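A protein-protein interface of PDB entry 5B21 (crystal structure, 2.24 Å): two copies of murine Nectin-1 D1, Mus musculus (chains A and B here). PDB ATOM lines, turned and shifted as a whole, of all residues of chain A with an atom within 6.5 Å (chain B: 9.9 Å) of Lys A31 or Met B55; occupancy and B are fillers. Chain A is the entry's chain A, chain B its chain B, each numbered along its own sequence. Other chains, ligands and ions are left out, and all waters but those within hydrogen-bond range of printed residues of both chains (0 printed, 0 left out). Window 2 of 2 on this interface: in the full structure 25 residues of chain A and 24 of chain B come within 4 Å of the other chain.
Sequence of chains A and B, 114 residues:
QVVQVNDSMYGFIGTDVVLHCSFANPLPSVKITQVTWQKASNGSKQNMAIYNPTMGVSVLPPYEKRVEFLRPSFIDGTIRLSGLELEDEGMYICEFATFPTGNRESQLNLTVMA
No residue of chain B comes within 4 Å of Val A30.
Of chain B, only Met B55 comes within 4 Å of Lys A31.
No residue of chain B comes within 4 Å of Ile A32.
Printed residues of chain B within 4 Å of Thr A33: Thr B33 (3.6 Å), Gln B34 (3.4 Å) and Asn B52 (3.5 Å).
Printed residues of chain B within 4 Å of Ala A97: Gln B34.
Thr A98 touches just one residue of chain B: Gln B34.
Phe A99 touches just these residues of chain B: Gln B34, Ile B50, Asn B52, Met B55, Gly B56, Val B57 and Ser B58.
Printed residues of chain A within 4 Å of Gln B34: Thr A33 (3.4 Å), Ala A97 (3.7 Å), Thr A98 (3.3 Å) and Phe A99 (3.3 Å).
Printed residues of chain A within 4 Å of Ile B50: Phe A99 and Pro A100.
Met B55 touches just these residues of chain A: Lys A31 and Phe A99.
Of the printed residues of chain A, Ser B58 touches Phe A99 and Pro A100.
The nearest residue of chain B that does not touch Lys A31 is Gln B34 (5.3 Å).
The nearest printed residue of chain B that does not touch Ala A97 is Thr B33 (6.2 Å).
Of the 14 printed residues of chain A, 7 touch a printed residue of chain B.
Printed residues of chain A that touch a printed residue of chain B: Lys A31, Thr A33, Gln A34, Ala A97, Thr A98, Phe A99 and Pro A100.
Hydrophobic or aromatic side chains of chain A within 4 Å of the printed part of chain B: Ala A97, Phe A99 and Pro A100.
Along chain A the printed residues that touch a printed residue of chain B span positions 31 to 100.
Hydrophobic or aromatic side chains of chain B within 4 Å of the printed part of chain A: Ile B50 and Met B55.
Among the printed residues, 16 pairs touch across the chains.
Among the printed residues, no Asp or Glu carboxylate lies within 4 Å of a Lys or Arg side-chain nitrogen of the other chain.
OE1 of Gln A34 sits at hydrogen-bond distance from OG1 of Thr B33, 3.2 Å away.
The backbone carbonyl oxygen of Thr A98 sits close to the side-chain amide oxygen of Gln B34.
OG of Ser B58 is in hydrogen-bond range of O of Pro A100, at 3.0 Å.
Met B55 touches Lys A31 (SD to CE, 3.6 Å).
OG1 of Thr A33 touches CG2 of Thr B33 (3.6 Å).
CG2 of Thr A33 touches OE1 of Gln B34, 3.4 Å away.
Thr A33 touches Asn B52 (CG2 to ND2, 3.5 Å).
Ala A97 touches Gln B34.
Gln B34 touches Phe A99 (OE1 to CB, 3.3 Å).
Phe A99 touches Met B55 (CZ to O, 3.4 Å).
Gly B56 touches Phe A99 (O to CE2, 3.4 Å).
Val B57 touches Phe A99.
Ile B50 touches Pro A100.
The backbone NH (N) of Lys A31 lies within hydrogen-bond range of the backbone carbonyl oxygen (O) of Phe A99 (2.9 Å).
The backbone carbonyl oxygen (O) of Gln A34 sits at hydrogen-bond distance from the backbone NH (N) of Ala A97, at 3.0 Å.
The backbone carbonyl oxygen (O) of Thr B33 sits close to the side-chain amide oxygen (OD1) of Asn B52 (3.3 Å).
The side-chain amide oxygen of Gln B34 sits at hydrogen-bond distance from the side-chain amide nitrogen of Asn B52, 3.2 Å away.
O of Ser B58 lies within hydrogen-bond range of N of Ile B50.
The side-chain amide oxygen of Asn B52 sits close to the backbone NH of Thr B54 (3.1 Å).
Thr B33 touches its own counterpart, Thr A33.
Thr A33 touches Gln B34, and with the chains exchanged Gln A34 touches Thr B33.
3 positions are printed for both chains.
Of the 16 pairs that touch across the chains among the printed residues, 3 have their exchanged pair printed and touching as well.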
ATOM      1  N   PRO A  26      10.956  14.714 -14.136  1.00  0.00           N
ATOM      2  CA  PRO A  26      10.537  15.686 -15.147  1.00  0.00           C
ATOM      3  C   PRO A  26       9.563  15.048 -16.131  1.00  0.00           C
ATOM      4  O   PRO A  26       9.893  14.038 -16.754  1.00  0.00           O
ATOM      5  CB  PRO A  26      11.849  16.075 -15.831  1.00  0.00           C
ATOM      6  CG  PRO A  26      12.748  14.906 -15.614  1.00  0.00           C
ATOM      7  CD  PRO A  26      12.378  14.354 -14.267  1.00  0.00           C
ATOM      8  N   LEU A  27       8.372  15.624 -16.246  1.00  0.00           N
ATOM      9  CA  LEU A  27       7.358  15.116 -17.162  1.00  0.00           C
ATOM     10  C   LEU A  27       7.878  15.134 -18.598  1.00  0.00           C
ATOM     11  O   LEU A  27       8.748  15.942 -18.929  1.00  0.00           O
ATOM     12  CB  LEU A  27       6.076  15.945 -17.045  1.00  0.00           C
ATOM     13  CG  LEU A  27       5.514  16.119 -15.632  1.00  0.00           C
ATOM     14  CD1 LEU A  27       4.198  16.880 -15.667  1.00  0.00           C
ATOM     15  CD2 LEU A  27       5.344  14.772 -14.947  1.00  0.00           C
ATOM     16  N   PRO A  28       7.357  14.239 -19.454  1.00  0.00           N
ATOM     17  CA  PRO A  28       7.760  14.221 -20.865  1.00  0.00           C
ATOM     18  C   PRO A  28       7.500  15.557 -21.557  1.00  0.00           C
ATOM     19  O   PRO A  28       8.127  15.862 -22.571  1.00  0.00           O
ATOM     20  CB  PRO A  28       6.892  13.108 -21.470  1.00  0.00           C
ATOM     21  CG  PRO A  28       5.781  12.896 -20.488  1.00  0.00           C
ATOM     22  CD  PRO A  28       6.382  13.177 -19.151  1.00  0.00           C
ATOM     23  N   SER A  29       6.579  16.340 -21.003  1.00  0.00           N
ATOM     24  CA  SER A  29       6.317  17.689 -21.483  1.00  0.00           C
ATOM     25  C   SER A  29       7.434  18.640 -21.063  1.00  0.00           C
ATOM     26  O   SER A  29       7.809  19.545 -21.811  1.00  0.00           O
ATOM     27  CB  SER A  29       4.971  18.190 -20.955  1.00  0.00           C
ATOM     28  OG  SER A  29       4.633  19.445 -21.519  1.00  0.00           O
ATOM     29  N   VAL A  30       7.968  18.422 -19.866  1.00  0.00           N
ATOM     30  CA  VAL A  30       8.985  19.301 -19.297  1.00  0.00           C
ATOM     31  C   VAL A  30      10.360  19.092 -19.928  1.00  0.00           C
ATOM     32  O   VAL A  30      10.863  17.971 -19.995  1.00  0.00           O
ATOM     33  CB  VAL A  30       9.107  19.098 -17.773  1.00  0.00           C
ATOM     34  CG1 VAL A  30      10.139  20.052 -17.188  1.00  0.00           C
ATOM     35  CG2 VAL A  30       7.756  19.291 -17.101  1.00  0.00           C
ATOM     36  N   LYS A  31      10.960  20.186 -20.389  1.00  0.00           N
ATOM     37  CA  LYS A  31      12.310  20.164 -20.937  1.00  0.00           C
ATOM     38  C   LYS A  31      13.250  21.032 -20.108  1.00  0.00           C
ATOM     39  O   LYS A  31      12.975  22.208 -19.868  1.00  0.00           O
ATOM     40  CB  LYS A  31      12.317  20.644 -22.390  1.00  0.00           C
ATOM     41  CG  LYS A  31      11.588  19.736 -23.366  1.00  0.00           C
ATOM     42  CD  LYS A  31      12.379  19.569 -24.661  1.00  0.00           C
ATOM     43  CE  LYS A  31      13.218  20.801 -24.976  1.00  0.00           C
ATOM     44  NZ  LYS A  31      14.032  20.631 -26.211  1.00  0.00           N
ATOM     45  N   ILE A  32      14.359  20.443 -19.672  1.00  0.00           N
ATOM     46  CA  ILE A  32      15.370  21.172 -18.916  1.00  0.00           C
ATOM     47  C   ILE A  32      16.323  21.880 -19.873  1.00  0.00           C
ATOM     48  O   ILE A  32      16.882  21.261 -20.778  1.00  0.00           O
ATOM     49  CB  ILE A  32      16.172  20.244 -17.977  1.00  0.00           C
ATOM     50  CG1 ILE A  32      15.320  19.815 -16.778  1.00  0.00           C
ATOM     51  CG2 ILE A  32      17.432  20.936 -17.486  1.00  0.00           C
ATOM     52  CD1 ILE A  32      14.394  18.646 -17.047  1.00  0.00           C
ATOM     53  N   THR A  33      16.502  23.181 -19.671  1.00  0.00           N
ATOM     54  CA  THR A  33      17.324  23.986 -20.563  1.00  0.00           C
ATOM     55  C   THR A  33      18.692  24.297 -19.961  1.00  0.00           C
ATOM     56  O   THR A  33      19.675  24.437 -20.689  1.00  0.00           O
ATOM     57  CB  THR A  33      16.625  25.313 -20.924  1.00  0.00           C
ATOM     58  OG1 THR A  33      16.680  26.210 -19.808  1.00  0.00           O
ATOM     59  CG2 THR A  33      15.172  25.067 -21.309  1.00  0.00           C
ATOM     60  N   GLN A  34      18.753  24.404 -18.636  1.00  0.00           N
ATOM     61  CA  GLN A  34      19.997  24.768 -17.961  1.00  0.00           C
ATOM     62  C   GLN A  34      19.961  24.449 -16.467  1.00  0.00           C
ATOM     63  O   GLN A  34      18.896  24.432 -15.851  1.00  0.00           O
ATOM     64  CB  GLN A  34      20.289  26.257 -18.169  1.00  0.00           C
ATOM     65  CG  GLN A  34      21.694  26.687 -17.784  1.00  0.00           C
ATOM     66  CD  GLN A  34      21.923  28.172 -17.983  1.00  0.00           C
ATOM     67  OE1 GLN A  34      22.043  28.648 -19.112  1.00  0.00           O
ATOM     68  NE2 GLN A  34      21.982  28.914 -16.883  1.00  0.00           N
ATOM     69  N   ALA A  97      16.271  25.597 -14.862  1.00  0.00           N
ATOM     70  CA  ALA A  97      15.441  26.380 -15.768  1.00  0.00           C
ATOM     71  C   ALA A  97      14.741  25.448 -16.748  1.00  0.00           C
ATOM     72  O   ALA A  97      15.389  24.816 -17.578  1.00  0.00           O
ATOM     73  CB  ALA A  97      16.278  27.409 -16.509  1.00  0.00           C
ATOM     74  N   THR A  98      13.420  25.355 -16.646  1.00  0.00           N
ATOM     75  CA  THR A  98      12.663  24.417 -17.467  1.00  0.00           C
ATOM     76  C   THR A  98      11.575  25.091 -18.297  1.00  0.00           C
ATOM     77  O   THR A  98      11.152  26.210 -18.007  1.00  0.00           O
ATOM     78  CB  THR A  98      12.006  23.321 -16.605  1.00  0.00           C
ATOM     79  OG1 THR A  98      11.002  23.907 -15.766  1.00  0.00           O
ATOM     80  CG2 THR A  98      13.045  22.620 -15.742  1.00  0.00           C
ATOM     81  N   PHE A  99      11.127  24.389 -19.332  1.00  0.00           N
ATOM     82  CA  PHE A  99      10.056  24.864 -20.197  1.00  0.00           C
ATOM     83  C   PHE A  99       9.047  23.737 -20.395  1.00  0.00           C
ATOM     84  O   PHE A  99       9.435  22.607 -20.674  1.00  0.00           O
ATOM     85  CB  PHE A  99      10.618  25.332 -21.542  1.00  0.00           C
ATOM     86  CG  PHE A  99       9.651  26.141 -22.363  1.00  0.00           C
ATOM     87  CD1 PHE A  99       8.700  25.518 -23.157  1.00  0.00           C
ATOM     88  CD2 PHE A  99       9.705  27.525 -22.353  1.00  0.00           C
ATOM     89  CE1 PHE A  99       7.814  26.261 -23.915  1.00  0.00           C
ATOM     90  CE2 PHE A  99       8.822  28.273 -23.111  1.00  0.00           C
ATOM     91  CZ  PHE A  99       7.876  27.640 -23.892  1.00  0.00           C
ATOM     92  N   PRO A 100       7.747  24.038 -20.263  1.00  0.00           N
ATOM     93  CA  PRO A 100       7.157  25.350 -19.993  1.00  0.00           C
ATOM     94  C   PRO A 100       6.895  25.616 -18.510  1.00  0.00           C
ATOM     95  O   PRO A 100       6.229  26.595 -18.177  1.00  0.00           O
ATOM     96  CB  PRO A 100       5.840  25.278 -20.760  1.00  0.00           C
ATOM     97  CG  PRO A 100       5.432  23.849 -20.610  1.00  0.00           C
ATOM     98  CD  PRO A 100       6.710  23.035 -20.568  1.00  0.00           C
ATOM     99  N   THR A 101       7.412  24.758 -17.637  1.00  0.00           N
ATOM    100  CA  THR A 101       7.122  24.855 -16.208  1.00  0.00           C
ATOM    101  C   THR A 101       7.848  26.012 -15.524  1.00  0.00           C
ATOM    102  O   THR A 101       7.347  26.577 -14.553  1.00  0.00           O
ATOM    103  CB  THR A 101       7.482  23.548 -15.477  1.00  0.00           C
ATOM    104  OG1 THR A 101       8.766  23.091 -15.917  1.00  0.00           O
ATOM    105  CG2 THR A 101       6.445  22.476 -15.768  1.00  0.00           C
ATOM    106  N   ILE B  32      21.696  33.840 -24.117  1.00  0.00           N
ATOM    107  CA  ILE B  32      20.518  33.806 -23.255  1.00  0.00           C
ATOM    108  C   ILE B  32      19.671  32.573 -23.561  1.00  0.00           C
ATOM    109  O   ILE B  32      19.279  32.346 -24.706  1.00  0.00           O
ATOM    110  CB  ILE B  32      19.655  35.083 -23.407  1.00  0.00           C
ATOM    111  CG1 ILE B  32      20.236  36.237 -22.583  1.00  0.00           C
ATOM    112  CG2 ILE B  32      18.226  34.827 -22.955  1.00  0.00           C
ATOM    113  CD1 ILE B  32      21.483  36.868 -23.166  1.00  0.00           C
ATOM    114  N   THR B  33      19.395  31.779 -22.532  1.00  0.00           N
ATOM    115  CA  THR B  33      18.656  30.534 -22.703  1.00  0.00           C
ATOM    116  C   THR B  33      17.163  30.712 -22.444  1.00  0.00           C
ATOM    117  O   THR B  33      16.333  30.182 -23.179  1.00  0.00           O
ATOM    118  CB  THR B  33      19.194  29.432 -21.771  1.00  0.00           C
ATOM    119  OG1 THR B  33      20.624  29.384 -21.860  1.00  0.00           O
ATOM    120  CG2 THR B  33      18.619  28.080 -22.158  1.00  0.00           C
ATOM    121  N   GLN B  34      16.826  31.457 -21.395  1.00  0.00           N
ATOM    122  CA  GLN B  34      15.429  31.679 -21.038  1.00  0.00           C
ATOM    123  C   GLN B  34      15.205  32.984 -20.281  1.00  0.00           C
ATOM    124  O   GLN B  34      16.088  33.470 -19.573  1.00  0.00           O
ATOM    125  CB  GLN B  34      14.900  30.516 -20.196  1.00  0.00           C
ATOM    126  CG  GLN B  34      14.132  29.470 -20.983  1.00  0.00           C
ATOM    127  CD  GLN B  34      13.492  28.424 -20.094  1.00  0.00           C
ATOM    128  OE1 GLN B  34      12.861  27.484 -20.577  1.00  0.00           O
ATOM    129  NE2 GLN B  34      13.647  28.583 -18.784  1.00  0.00           N
ATOM    130  N   VAL B  35      14.011  33.543 -20.446  1.00  0.00           N
ATOM    131  CA  VAL B  35      13.552  34.665 -19.642  1.00  0.00           C
ATOM    132  C   VAL B  35      12.386  34.176 -18.793  1.00  0.00           C
ATOM    133  O   VAL B  35      11.461  33.559 -19.311  1.00  0.00           O
ATOM    134  CB  VAL B  35      13.108  35.857 -20.508  1.00  0.00           C
ATOM    135  CG1 VAL B  35      13.024  37.119 -19.667  1.00  0.00           C
ATOM    136  CG2 VAL B  35      14.068  36.053 -21.669  1.00  0.00           C
ATOM    137  N   ILE B  50       7.373  32.339 -19.058  1.00  0.00           N
ATOM    138  CA  ILE B  50       8.676  31.951 -19.588  1.00  0.00           C
ATOM    139  C   ILE B  50       8.760  32.165 -21.095  1.00  0.00           C
ATOM    140  O   ILE B  50       7.942  31.640 -21.845  1.00  0.00           O
ATOM    141  CB  ILE B  50       9.011  30.460 -19.309  1.00  0.00           C
ATOM    142  CG1 ILE B  50       8.941  30.130 -17.815  1.00  0.00           C
ATOM    143  CG2 ILE B  50      10.385  30.114 -19.862  1.00  0.00           C
ATOM    144  CD1 ILE B  50       7.600  29.574 -17.367  1.00  0.00           C
ATOM    145  N   TYR B  51       9.749  32.932 -21.537  1.00  0.00           N
ATOM    146  CA  TYR B  51      10.066  32.990 -22.956  1.00  0.00           C
ATOM    147  C   TYR B  51      11.372  32.264 -23.243  1.00  0.00           C
ATOM    148  O   TYR B  51      12.407  32.560 -22.647  1.00  0.00           O
ATOM    149  CB  TYR B  51      10.162  34.430 -23.459  1.00  0.00           C
ATOM    150  CG  TYR B  51      10.633  34.502 -24.894  1.00  0.00           C
ATOM    151  CD1 TYR B  51       9.785  34.161 -25.938  1.00  0.00           C
ATOM    152  CD2 TYR B  51      11.932  34.887 -25.204  1.00  0.00           C
ATOM    153  CE1 TYR B  51      10.211  34.212 -27.253  1.00  0.00           C
ATOM    154  CE2 TYR B  51      12.367  34.941 -26.516  1.00  0.00           C
ATOM    155  CZ  TYR B  51      11.502  34.603 -27.536  1.00  0.00           C
ATOM    156  OH  TYR B  51      11.928  34.656 -28.843  1.00  0.00           O
ATOM    157  N   ASN B  52      11.310  31.311 -24.162  1.00  0.00           N
ATOM    158  CA  ASN B  52      12.493  30.600 -24.616  1.00  0.00           C
ATOM    159  C   ASN B  52      12.689  30.855 -26.104  1.00  0.00           C
ATOM    160  O   ASN B  52      11.784  30.609 -26.899  1.00  0.00           O
ATOM    161  CB  ASN B  52      12.362  29.102 -24.327  1.00  0.00           C
ATOM    162  CG  ASN B  52      13.673  28.353 -24.485  1.00  0.00           C
ATOM    163  OD1 ASN B  52      14.444  28.602 -25.410  1.00  0.00           O
ATOM    164  ND2 ASN B  52      13.929  27.421 -23.574  1.00  0.00           N
ATOM    165  N   PRO B  53      13.872  31.364 -26.483  1.00  0.00           N
ATOM    166  CA  PRO B  53      14.217  31.691 -27.873  1.00  0.00           C
ATOM    167  C   PRO B  53      13.942  30.559 -28.864  1.00  0.00           C
ATOM    168  O   PRO B  53      13.789  30.821 -30.057  1.00  0.00           O
ATOM    169  CB  PRO B  53      15.717  31.980 -27.794  1.00  0.00           C
ATOM    170  CG  PRO B  53      15.910  32.509 -26.420  1.00  0.00           C
ATOM    171  CD  PRO B  53      14.944  31.752 -25.549  1.00  0.00           C
ATOM    172  N   THR B  54      13.874  29.324 -28.378  1.00  0.00           N
ATOM    173  CA  THR B  54      13.658  28.173 -29.246  1.00  0.00           C
ATOM    174  C   THR B  54      12.351  27.442 -28.944  1.00  0.00           C
ATOM    175  O   THR B  54      11.758  26.828 -29.831  1.00  0.00           O
ATOM    176  CB  THR B  54      14.819  27.166 -29.135  1.00  0.00           C
ATOM    177  OG1 THR B  54      14.869  26.637 -27.804  1.00  0.00           O
ATOM    178  CG2 THR B  54      16.143  27.840 -29.460  1.00  0.00           C
ATOM    179  N   MET B  55      11.904  27.511 -27.694  1.00  0.00           N
ATOM    180  CA  MET B  55      10.729  26.756 -27.264  1.00  0.00           C
ATOM    181  C   MET B  55       9.438  27.568 -27.346  1.00  0.00           C
ATOM    182  O   MET B  55       8.344  27.016 -27.226  1.00  0.00           O
ATOM    183  CB  MET B  55      10.923  26.245 -25.835  1.00  0.00           C
ATOM    184  CG  MET B  55      12.076  25.270 -25.675  1.00  0.00           C
ATOM    185  SD  MET B  55      11.735  23.680 -26.451  1.00  0.00           S
ATOM    186  CE  MET B  55      10.386  23.090 -25.430  1.00  0.00           C
ATOM    187  N   GLY B  56       9.565  28.874 -27.547  1.00  0.00           N
ATOM    188  CA  GLY B  56       8.404  29.737 -27.670  1.00  0.00           C
ATOM    189  C   GLY B  56       7.994  30.392 -26.365  1.00  0.00           C
ATOM    190  O   GLY B  56       8.826  30.642 -25.493  1.00  0.00           O
ATOM    191  N   VAL B  57       6.700  30.666 -26.229  1.00  0.00           N
ATOM    192  CA  VAL B  57       6.184  31.376 -25.065  1.00  0.00           C
ATOM    193  C   VAL B  57       5.298  30.482 -24.202  1.00  0.00           C
ATOM    194  O   VAL B  57       4.487  29.709 -24.712  1.00  0.00           O
ATOM    195  CB  VAL B  57       5.385  32.630 -25.484  1.00  0.00           C
ATOM    196  CG1 VAL B  57       4.896  33.395 -24.261  1.00  0.00           C
ATOM    197  CG2 VAL B  57       6.236  33.527 -26.369  1.00  0.00           C
ATOM    198  N   SER B  58       5.473  30.593 -22.890  1.00  0.00           N
ATOM    199  CA  SER B  58       4.655  29.870 -21.929  1.00  0.00           C
ATOM    200  C   SER B  58       4.144  30.806 -20.843  1.00  0.00           C
ATOM    201  O   SER B  58       4.898  31.593 -20.280  1.00  0.00           O
ATOM    202  CB  SER B  58       5.448  28.727 -21.297  1.00  0.00           C
ATOM    203  OG  SER B  58       4.737  28.165 -20.208  1.00  0.00           O
ATOM    204  N   VAL B  59       2.848  30.724 -20.566  1.00  0.00           N
ATOM    205  CA  VAL B  59       2.250  31.477 -19.476  1.00  0.00           C
ATOM    206  C   VAL B  59       1.591  30.483 -18.534  1.00  0.00           C
ATOM    207  O   VAL B  59       0.897  29.570 -18.972  1.00  0.00           O
ATOM    208  CB  VAL B  59       1.214  32.505 -19.976  1.00  0.00           C
ATOM    209  CG1 VAL B  59       0.903  33.522 -18.891  1.00  0.00           C
ATOM    210  CG2 VAL B  59       1.719  33.204 -21.229  1.00  0.00           C
